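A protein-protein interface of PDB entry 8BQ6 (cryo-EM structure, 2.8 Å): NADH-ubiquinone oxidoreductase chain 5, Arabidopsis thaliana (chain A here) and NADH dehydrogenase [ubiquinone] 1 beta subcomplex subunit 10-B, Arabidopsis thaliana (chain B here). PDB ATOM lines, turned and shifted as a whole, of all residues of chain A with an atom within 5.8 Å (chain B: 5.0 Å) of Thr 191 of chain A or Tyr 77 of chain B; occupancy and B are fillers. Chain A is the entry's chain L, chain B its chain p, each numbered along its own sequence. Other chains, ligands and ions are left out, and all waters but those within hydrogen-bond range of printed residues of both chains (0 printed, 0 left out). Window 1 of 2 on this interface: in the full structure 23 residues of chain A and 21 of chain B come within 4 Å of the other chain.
O of Gln 190 of chain A lies within hydrogen-bond range of NH1 of Arg 52 of chain B (2.8 Å).
The side-chain hydroxyl (OH) of Tyr 77 of chain B sits at hydrogen-bond distance from the backbone carbonyl oxygen (O) of Gln 190 of chain A (3.4 Å).
The backbone carbonyl oxygen (O) of Met 69 of chain A is in hydrogen-bond range of the guanidinium group (NH1) of Arg 52 of chain B (3.2 Å).
OD1 of Asp 71 of chain A is in salt-bridge range of NH1 of Arg 52 of chain B, 3.7 Å away.
O of Phe 189 of chain A lies within hydrogen-bond range of OH of Tyr 77 of chain B, 2.6 Å away.
The backbone carbonyl oxygen of Tyr 77 of chain B sits at hydrogen-bond distance from the side-chain hydroxyl of Ser 80 of chain B, 2.8 Å away.
SG of Cys 200 of chain A sits at hydrogen-bond distance from O of Thr 196 of chain A (3.4 Å).
The backbone carbonyl oxygen of Leu 78 of chain B sits at hydrogen-bond distance from the side-chain hydroxyl of Thr 81 of chain B, 3.1 Å away.
OG1 of Thr 191 of chain A lies within hydrogen-bond range of N of Asp 193 of chain A (2.9 Å).
The backbone NH (N) of Thr 196 of chain A sits at hydrogen-bond distance from the side-chain carboxylate (OD2) of Asp 193 of chain A (2.8 Å).
OG1 of Thr 191 of chain A lies within hydrogen-bond range of OD1 of Asp 71 of chain A (3.5 Å).
Among the printed residues, pairs that only touch across the chains: Met 69 of chain A with Ala 48 of chain B, Met 69 of chain A with Thr 81 of chain B, Gln 190 of chain A with Thr 81 of chain B, Thr 191 of chain A with Arg 52 of chain B, Thr 191 of chain A with Tyr 77 of chain B, Thr 196 of chain A with Arg 52 of chain B, Cys 200 of chain A with Val 74 of chain B and Cys 200 of chain A with Tyr 77 of chain B.
Printed residues of chain B within 4 Å of Met 69 of chain A: Ala 48, Arg 52 and Thr 81.
Of the printed residues of chain B, Gln 190 of chain A touches Arg 52 (2.8 Å), Tyr 77 (3.4 Å) and Thr 81 (3.97 Å).
Of chain B, only Arg 52 and Tyr 77 come within 4 Å of Thr 191 of chain A.
Asp 193 of chain A touches none of the printed residues of chain B.
Printed residues of chain A within 4 Å of Ala 48 of chain B: Met 69.
Printed residues of chain A within 4 Å of Val 74 of chain B: Cys 200.
Of the printed residues of chain A, Tyr 77 of chain B touches Phe 189 (2.6 Å), Gln 190 (3.4 Å), Thr 191 (3.5 Å) and Cys 200 (3.9 Å).
Printed residues of chain A within 4 Å of Thr 81 of chain B: Met 69 and Gln 190.
The nearest printed residue of chain B that does not touch Thr 191 of chain A is Thr 81 of chain B (6.9 Å).
Printed residues of chain A that touch a printed residue of chain B: Met 69, Asp 71, Phe 189, Gln 190, Thr 191, Thr 196 and Cys 200.
Printed residues of chain B that touch a printed residue of chain A: Ala 48, Arg 52, Val 74, Tyr 77 and Thr 81.
Hydrophobic or aromatic side chains of chain B that line the printed part of chain A: Ala 48, Val 74 and Tyr 77.
Among the printed residues, 13 pairs touch across the chains.
Among the printed residues, Asp or Glu carboxylates within 4 Å of a Lys or Arg side-chain nitrogen of the other chain: Asp 71 of chain A with Arg 52 of chain B (3.7 Å).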
ATOM      1  N   MET A  69     -21.093   4.911  14.474  1.00  0.00           N
ATOM      2  CA  MET A  69     -22.047   4.524  15.509  1.00  0.00           C
ATOM      3  C   MET A  69     -21.971   5.435  16.729  1.00  0.00           C
ATOM      4  O   MET A  69     -22.905   5.452  17.538  1.00  0.00           O
ATOM      5  CB  MET A  69     -21.821   3.070  15.917  1.00  0.00           C
ATOM      6  CG  MET A  69     -22.140   2.057  14.824  1.00  0.00           C
ATOM      7  SD  MET A  69     -23.897   1.941  14.443  1.00  0.00           S
ATOM      8  CE  MET A  69     -24.426   0.794  15.706  1.00  0.00           C
ATOM      9  N   ASP A  71     -22.647   8.401  18.851  1.00  0.00           N
ATOM     10  CA  ASP A  71     -23.837   9.274  18.692  1.00  0.00           C
ATOM     11  C   ASP A  71     -24.053  10.196  19.894  1.00  0.00           C
ATOM     12  O   ASP A  71     -25.228  10.431  20.240  1.00  0.00           O
ATOM     13  CB  ASP A  71     -25.068   8.389  18.475  1.00  0.00           C
ATOM     14  CG  ASP A  71     -25.322   7.391  19.601  1.00  0.00           C
ATOM     15  OD1 ASP A  71     -24.420   6.584  19.898  1.00  0.00           O
ATOM     16  OD2 ASP A  71     -26.426   7.427  20.175  1.00  0.00           O
ATOM     17  N   CYS A 185     -18.128   1.201  27.440  1.00  0.00           N
ATOM     18  CA  CYS A 185     -19.559   1.118  27.175  1.00  0.00           C
ATOM     19  C   CYS A 185     -19.836   1.164  25.682  1.00  0.00           C
ATOM     20  O   CYS A 185     -20.608   0.351  25.157  1.00  0.00           O
ATOM     21  CB  CYS A 185     -20.296   2.251  27.888  1.00  0.00           C
ATOM     22  SG  CYS A 185     -20.999   1.802  29.485  1.00  0.00           S
ATOM     23  N   PHE A 186     -19.204   2.104  24.976  1.00  0.00           N
ATOM     24  CA  PHE A 186     -19.464   2.234  23.550  1.00  0.00           C
ATOM     25  C   PHE A 186     -18.994   1.009  22.785  1.00  0.00           C
ATOM     26  O   PHE A 186     -19.658   0.563  21.846  1.00  0.00           O
ATOM     27  CB  PHE A 186     -18.795   3.476  22.976  1.00  0.00           C
ATOM     28  CG  PHE A 186     -18.939   3.574  21.495  1.00  0.00           C
ATOM     29  CD1 PHE A 186     -20.166   3.868  20.937  1.00  0.00           C
ATOM     30  CD2 PHE A 186     -17.875   3.321  20.658  1.00  0.00           C
ATOM     31  CE1 PHE A 186     -20.322   3.935  19.578  1.00  0.00           C
ATOM     32  CE2 PHE A 186     -18.033   3.392  19.299  1.00  0.00           C
ATOM     33  CZ  PHE A 186     -19.255   3.698  18.758  1.00  0.00           C
ATOM     34  N   THR A 187     -17.837   0.469  23.150  1.00  0.00           N
ATOM     35  CA  THR A 187     -17.310  -0.678  22.425  1.00  0.00           C
ATOM     36  C   THR A 187     -18.236  -1.881  22.556  1.00  0.00           C
ATOM     37  O   THR A 187     -18.397  -2.658  21.608  1.00  0.00           O
ATOM     38  CB  THR A 187     -15.904  -0.994  22.931  1.00  0.00           C
ATOM     39  OG1 THR A 187     -15.053   0.132  22.679  1.00  0.00           O
ATOM     40  CG2 THR A 187     -15.332  -2.207  22.231  1.00  0.00           C
ATOM     41  N   PHE A 189     -21.782  -1.906  23.580  1.00  0.00           N
ATOM     42  CA  PHE A 189     -23.148  -1.682  23.121  1.00  0.00           C
ATOM     43  C   PHE A 189     -23.241  -0.859  21.845  1.00  0.00           C
ATOM     44  O   PHE A 189     -24.350  -0.682  21.328  1.00  0.00           O
ATOM     45  CB  PHE A 189     -23.968  -0.977  24.203  1.00  0.00           C
ATOM     46  CG  PHE A 189     -24.032  -1.721  25.493  1.00  0.00           C
ATOM     47  CD1 PHE A 189     -24.828  -2.842  25.619  1.00  0.00           C
ATOM     48  CD2 PHE A 189     -23.308  -1.291  26.587  1.00  0.00           C
ATOM     49  CE1 PHE A 189     -24.892  -3.524  26.810  1.00  0.00           C
ATOM     50  CE2 PHE A 189     -23.366  -1.971  27.777  1.00  0.00           C
ATOM     51  CZ  PHE A 189     -24.159  -3.089  27.891  1.00  0.00           C
ATOM     52  N   GLN A 190     -22.121  -0.339  21.346  1.00  0.00           N
ATOM     53  CA  GLN A 190     -22.092   0.507  20.152  1.00  0.00           C
ATOM     54  C   GLN A 190     -22.984   1.737  20.295  1.00  0.00           C
ATOM     55  O   GLN A 190     -23.598   2.188  19.325  1.00  0.00           O
ATOM     56  CB  GLN A 190     -22.456  -0.295  18.901  1.00  0.00           C
ATOM     57  CG  GLN A 190     -21.400  -1.326  18.536  1.00  0.00           C
ATOM     58  CD  GLN A 190     -20.091  -0.686  18.124  1.00  0.00           C
ATOM     59  OE1 GLN A 190     -19.995  -0.077  17.060  1.00  0.00           O
ATOM     60  NE2 GLN A 190     -19.076  -0.815  18.970  1.00  0.00           N
ATOM     61  N   THR A 191     -23.037   2.307  21.497  1.00  0.00           N
ATOM     62  CA  THR A 191     -23.809   3.516  21.742  1.00  0.00           C
ATOM     63  C   THR A 191     -23.447   4.071  23.111  1.00  0.00           C
ATOM     64  O   THR A 191     -23.053   3.332  24.015  1.00  0.00           O
ATOM     65  CB  THR A 191     -25.315   3.256  21.673  1.00  0.00           C
ATOM     66  OG1 THR A 191     -26.019   4.415  22.131  1.00  0.00           O
ATOM     67  CG2 THR A 191     -25.685   2.074  22.544  1.00  0.00           C
ATOM     68  N   VAL A 192     -23.648   5.385  23.253  1.00  0.00           N
ATOM     69  CA  VAL A 192     -23.436   6.040  24.572  1.00  0.00           C
ATOM     70  C   VAL A 192     -24.792   6.499  25.126  1.00  0.00           C
ATOM     71  O   VAL A 192     -24.787   7.049  26.230  1.00  0.00           O
ATOM     72  CB  VAL A 192     -22.437   7.209  24.459  1.00  0.00           C
ATOM     73  CG1 VAL A 192     -21.027   6.715  24.187  1.00  0.00           C
ATOM     74  CG2 VAL A 192     -22.862   8.230  23.416  1.00  0.00           C
ATOM     75  N   ASP A 193     -25.906   6.247  24.414  1.00  0.00           N
ATOM     76  CA  ASP A 193     -27.218   6.687  24.868  1.00  0.00           C
ATOM     77  C   ASP A 193     -27.658   5.882  26.087  1.00  0.00           C
ATOM     78  O   ASP A 193     -27.489   4.660  26.128  1.00  0.00           O
ATOM     79  CB  ASP A 193     -28.227   6.545  23.729  1.00  0.00           C
ATOM     80  CG  ASP A 193     -29.650   6.749  24.182  1.00  0.00           C
ATOM     81  OD1 ASP A 193     -30.108   7.908  24.202  1.00  0.00           O
ATOM     82  OD2 ASP A 193     -30.315   5.744  24.509  1.00  0.00           O
ATOM     83  N   THR A 196     -30.766   3.212  25.501  1.00  0.00           N
ATOM     84  CA  THR A 196     -30.411   2.029  24.723  1.00  0.00           C
ATOM     85  C   THR A 196     -29.558   1.066  25.541  1.00  0.00           C
ATOM     86  O   THR A 196     -29.788  -0.150  25.526  1.00  0.00           O
ATOM     87  CB  THR A 196     -29.696   2.439  23.436  1.00  0.00           C
ATOM     88  OG1 THR A 196     -30.532   3.331  22.692  1.00  0.00           O
ATOM     89  CG2 THR A 196     -29.373   1.224  22.586  1.00  0.00           C
ATOM     90  N   ILE A 197     -28.576   1.594  26.274  1.00  0.00           N
ATOM     91  CA  ILE A 197     -27.680   0.747  27.059  1.00  0.00           C
ATOM     92  C   ILE A 197     -28.449   0.012  28.148  1.00  0.00           C
ATOM     93  O   ILE A 197     -28.236  -1.184  28.382  1.00  0.00           O
ATOM     94  CB  ILE A 197     -26.537   1.590  27.651  1.00  0.00           C
ATOM     95  CG1 ILE A 197     -25.494   1.903  26.584  1.00  0.00           C
ATOM     96  CG2 ILE A 197     -25.891   0.887  28.835  1.00  0.00           C
ATOM     97  CD1 ILE A 197     -24.578   3.033  26.966  1.00  0.00           C
ATOM     98  N   CYS A 200     -30.365  -2.921  26.849  1.00  0.00           N
ATOM     99  CA  CYS A 200     -29.596  -4.045  26.335  1.00  0.00           C
ATOM    100  C   CYS A 200     -28.681  -4.678  27.371  1.00  0.00           C
ATOM    101  O   CYS A 200     -28.039  -5.686  27.067  1.00  0.00           O
ATOM    102  CB  CYS A 200     -28.749  -3.599  25.140  1.00  0.00           C
ATOM    103  SG  CYS A 200     -29.710  -3.038  23.733  1.00  0.00           S
ATOM    104  N   ALA B  48     -28.377  -0.156  11.809  1.00  0.00           N
ATOM    105  CA  ALA B  48     -28.300  -0.321  13.255  1.00  0.00           C
ATOM    106  C   ALA B  48     -28.768   0.928  13.988  1.00  0.00           C
ATOM    107  O   ALA B  48     -29.307   0.830  15.094  1.00  0.00           O
ATOM    108  CB  ALA B  48     -26.875  -0.682  13.668  1.00  0.00           C
ATOM    109  N   LEU B  51     -32.485   0.826  13.899  1.00  0.00           N
ATOM    110  CA  LEU B  51     -32.867  -0.195  14.866  1.00  0.00           C
ATOM    111  C   LEU B  51     -32.617   0.272  16.291  1.00  0.00           C
ATOM    112  O   LEU B  51     -33.302  -0.168  17.220  1.00  0.00           O
ATOM    113  CB  LEU B  51     -32.093  -1.483  14.595  1.00  0.00           C
ATOM    114  CG  LEU B  51     -32.502  -2.286  13.361  1.00  0.00           C
ATOM    115  CD1 LEU B  51     -31.942  -3.690  13.443  1.00  0.00           C
ATOM    116  CD2 LEU B  51     -34.013  -2.313  13.192  1.00  0.00           C
ATOM    117  N   ARG B  52     -31.634   1.153  16.484  1.00  0.00           N
ATOM    118  CA  ARG B  52     -31.328   1.632  17.826  1.00  0.00           C
ATOM    119  C   ARG B  52     -32.372   2.631  18.303  1.00  0.00           C
ATOM    120  O   ARG B  52     -32.712   2.665  19.492  1.00  0.00           O
ATOM    121  CB  ARG B  52     -29.929   2.240  17.847  1.00  0.00           C
ATOM    122  CG  ARG B  52     -29.576   2.982  19.110  1.00  0.00           C
ATOM    123  CD  ARG B  52     -28.101   3.305  19.113  1.00  0.00           C
ATOM    124  NE  ARG B  52     -27.755   4.313  18.121  1.00  0.00           N
ATOM    125  CZ  ARG B  52     -26.540   4.471  17.616  1.00  0.00           C
ATOM    126  NH1 ARG B  52     -25.548   3.658  17.940  1.00  0.00           N
ATOM    127  NH2 ARG B  52     -26.314   5.470  16.770  1.00  0.00           N
ATOM    128  N   VAL B  55     -35.209   0.598  19.853  1.00  0.00           N
ATOM    129  CA  VAL B  55     -34.934   0.135  21.212  1.00  0.00           C
ATOM    130  C   VAL B  55     -35.082   1.279  22.200  1.00  0.00           C
ATOM    131  O   VAL B  55     -35.617   1.111  23.302  1.00  0.00           O
ATOM    132  CB  VAL B  55     -33.535  -0.500  21.290  1.00  0.00           C
ATOM    133  CG1 VAL B  55     -33.127  -0.711  22.733  1.00  0.00           C
ATOM    134  CG2 VAL B  55     -33.519  -1.816  20.553  1.00  0.00           C
ATOM    135  N   LEU B  73     -36.723  -6.455  19.879  1.00  0.00           N
ATOM    136  CA  LEU B  73     -35.989  -5.343  19.277  1.00  0.00           C
ATOM    137  C   LEU B  73     -34.534  -5.321  19.729  1.00  0.00           C
ATOM    138  O   LEU B  73     -33.644  -4.953  18.953  1.00  0.00           O
ATOM    139  CB  LEU B  73     -36.659  -4.011  19.611  1.00  0.00           C
ATOM    140  CG  LEU B  73     -37.913  -3.614  18.836  1.00  0.00           C
ATOM    141  CD1 LEU B  73     -38.343  -2.212  19.218  1.00  0.00           C
ATOM    142  CD2 LEU B  73     -37.687  -3.719  17.340  1.00  0.00           C
ATOM    143  N   VAL B  74     -34.276  -5.682  20.988  1.00  0.00           N
ATOM    144  CA  VAL B  74     -32.906  -5.693  21.494  1.00  0.00           C
ATOM    145  C   VAL B  74     -32.081  -6.742  20.764  1.00  0.00           C
ATOM    146  O   VAL B  74     -30.904  -6.527  20.452  1.00  0.00           O
ATOM    147  CB  VAL B  74     -32.903  -5.935  23.014  1.00  0.00           C
ATOM    148  CG1 VAL B  74     -31.493  -6.189  23.512  1.00  0.00           C
ATOM    149  CG2 VAL B  74     -33.524  -4.760  23.737  1.00  0.00           C
ATOM    150  N   GLN B  75     -32.683  -7.902  20.498  1.00  0.00           N
ATOM    151  CA  GLN B  75     -31.981  -8.946  19.765  1.00  0.00           C
ATOM    152  C   GLN B  75     -31.614  -8.465  18.369  1.00  0.00           C
ATOM    153  O   GLN B  75     -30.505  -8.717  17.885  1.00  0.00           O
ATOM    154  CB  GLN B  75     -32.854 -10.200  19.703  1.00  0.00           C
ATOM    155  CG  GLN B  75     -32.188 -11.414  19.091  1.00  0.00           C
ATOM    156  CD  GLN B  75     -33.027 -12.667  19.204  1.00  0.00           C
ATOM    157  OE1 GLN B  75     -34.084 -12.657  19.827  1.00  0.00           O
ATOM    158  NE2 GLN B  75     -32.572 -13.748  18.585  1.00  0.00           N
ATOM    159  N   GLN B  76     -32.548  -7.792  17.700  1.00  0.00           N
ATOM    160  CA  GLN B  76     -32.299  -7.303  16.350  1.00  0.00           C
ATOM    161  C   GLN B  76     -31.205  -6.247  16.340  1.00  0.00           C
ATOM    162  O   GLN B  76     -30.328  -6.252  15.469  1.00  0.00           O
ATOM    163  CB  GLN B  76     -33.587  -6.737  15.771  1.00  0.00           C
ATOM    164  CG  GLN B  76     -34.678  -7.758  15.639  1.00  0.00           C
ATOM    165  CD  GLN B  76     -35.638  -7.397  14.546  1.00  0.00           C
ATOM    166  OE1 GLN B  76     -35.934  -8.208  13.674  1.00  0.00           O
ATOM    167  NE2 GLN B  76     -36.126  -6.163  14.575  1.00  0.00           N
ATOM    168  N   TYR B  77     -31.256  -5.314  17.291  1.00  0.00           N
ATOM    169  CA  TYR B  77     -30.229  -4.285  17.357  1.00  0.00           C
ATOM    170  C   TYR B  77     -28.863  -4.889  17.649  1.00  0.00           C
ATOM    171  O   TYR B  77     -27.870  -4.540  17.001  1.00  0.00           O
ATOM    172  CB  TYR B  77     -30.588  -3.246  18.417  1.00  0.00           C
ATOM    173  CG  TYR B  77     -29.430  -2.349  18.767  1.00  0.00           C
ATOM    174  CD1 TYR B  77     -29.018  -1.358  17.892  1.00  0.00           C
ATOM    175  CD2 TYR B  77     -28.742  -2.497  19.963  1.00  0.00           C
ATOM    176  CE1 TYR B  77     -27.964  -0.537  18.194  1.00  0.00           C
ATOM    177  CE2 TYR B  77     -27.677  -1.677  20.274  1.00  0.00           C
ATOM    178  CZ  TYR B  77     -27.295  -0.697  19.382  1.00  0.00           C
ATOM    179  OH  TYR B  77     -26.238   0.132  19.669  1.00  0.00           O
ATOM    180  N   LEU B  78     -28.794  -5.808  18.614  1.00  0.00           N
ATOM    181  CA  LEU B  78     -27.504  -6.372  18.997  1.00  0.00           C
ATOM    182  C   LEU B  78     -26.927  -7.259  17.900  1.00  0.00           C
ATOM    183  O   LEU B  78     -25.703  -7.374  17.781  1.00  0.00           O
ATOM    184  CB  LEU B  78     -27.646  -7.141  20.311  1.00  0.00           C
ATOM    185  CG  LEU B  78     -27.638  -6.282  21.581  1.00  0.00           C
ATOM    186  CD1 LEU B  78     -27.391  -7.132  22.809  1.00  0.00           C
ATOM    187  CD2 LEU B  78     -26.602  -5.172  21.497  1.00  0.00           C
ATOM    188  N   ASP B  79     -27.782  -7.886  17.090  1.00  0.00           N
ATOM    189  CA  ASP B  79     -27.291  -8.643  15.943  1.00  0.00           C
ATOM    190  C   ASP B  79     -26.791  -7.714  14.844  1.00  0.00           C
ATOM    191  O   ASP B  79     -25.803  -8.014  14.165  1.00  0.00           O
ATOM    192  CB  ASP B  79     -28.388  -9.567  15.418  1.00  0.00           C
ATOM    193  CG  ASP B  79     -28.563 -10.799  16.273  1.00  0.00           C
ATOM    194  OD1 ASP B  79     -28.528 -10.664  17.512  1.00  0.00           O
ATOM    195  OD2 ASP B  79     -28.738 -11.900  15.711  1.00  0.00           O
ATOM    196  N   SER B  80     -27.463  -6.578  14.650  1.00  0.00           N
ATOM    197  CA  SER B  80     -27.041  -5.650  13.609  1.00  0.00           C
ATOM    198  C   SER B  80     -25.742  -4.943  13.971  1.00  0.00           C
ATOM    199  O   SER B  80     -24.992  -4.533  13.078  1.00  0.00           O
ATOM    200  CB  SER B  80     -28.136  -4.620  13.344  1.00  0.00           C
ATOM    201  OG  SER B  80     -28.140  -3.632  14.356  1.00  0.00           O
ATOM    202  N   THR B  81     -25.465  -4.773  15.267  1.00  0.00           N
ATOM    203  CA  THR B  81     -24.250  -4.079  15.680  1.00  0.00           C
ATOM    204  C   THR B  81     -23.033  -4.983  15.718  1.00  0.00           C
ATOM    205  O   THR B  81     -21.909  -4.481  15.617  1.00  0.00           O
ATOM    206  CB  THR B  81     -24.417  -3.435  17.056  1.00  0.00           C
ATOM    207  OG1 THR B  81     -24.836  -4.421  18.006  1.00  0.00           O
ATOM    208  CG2 THR B  81     -25.423  -2.328  16.993  1.00  0.00           C
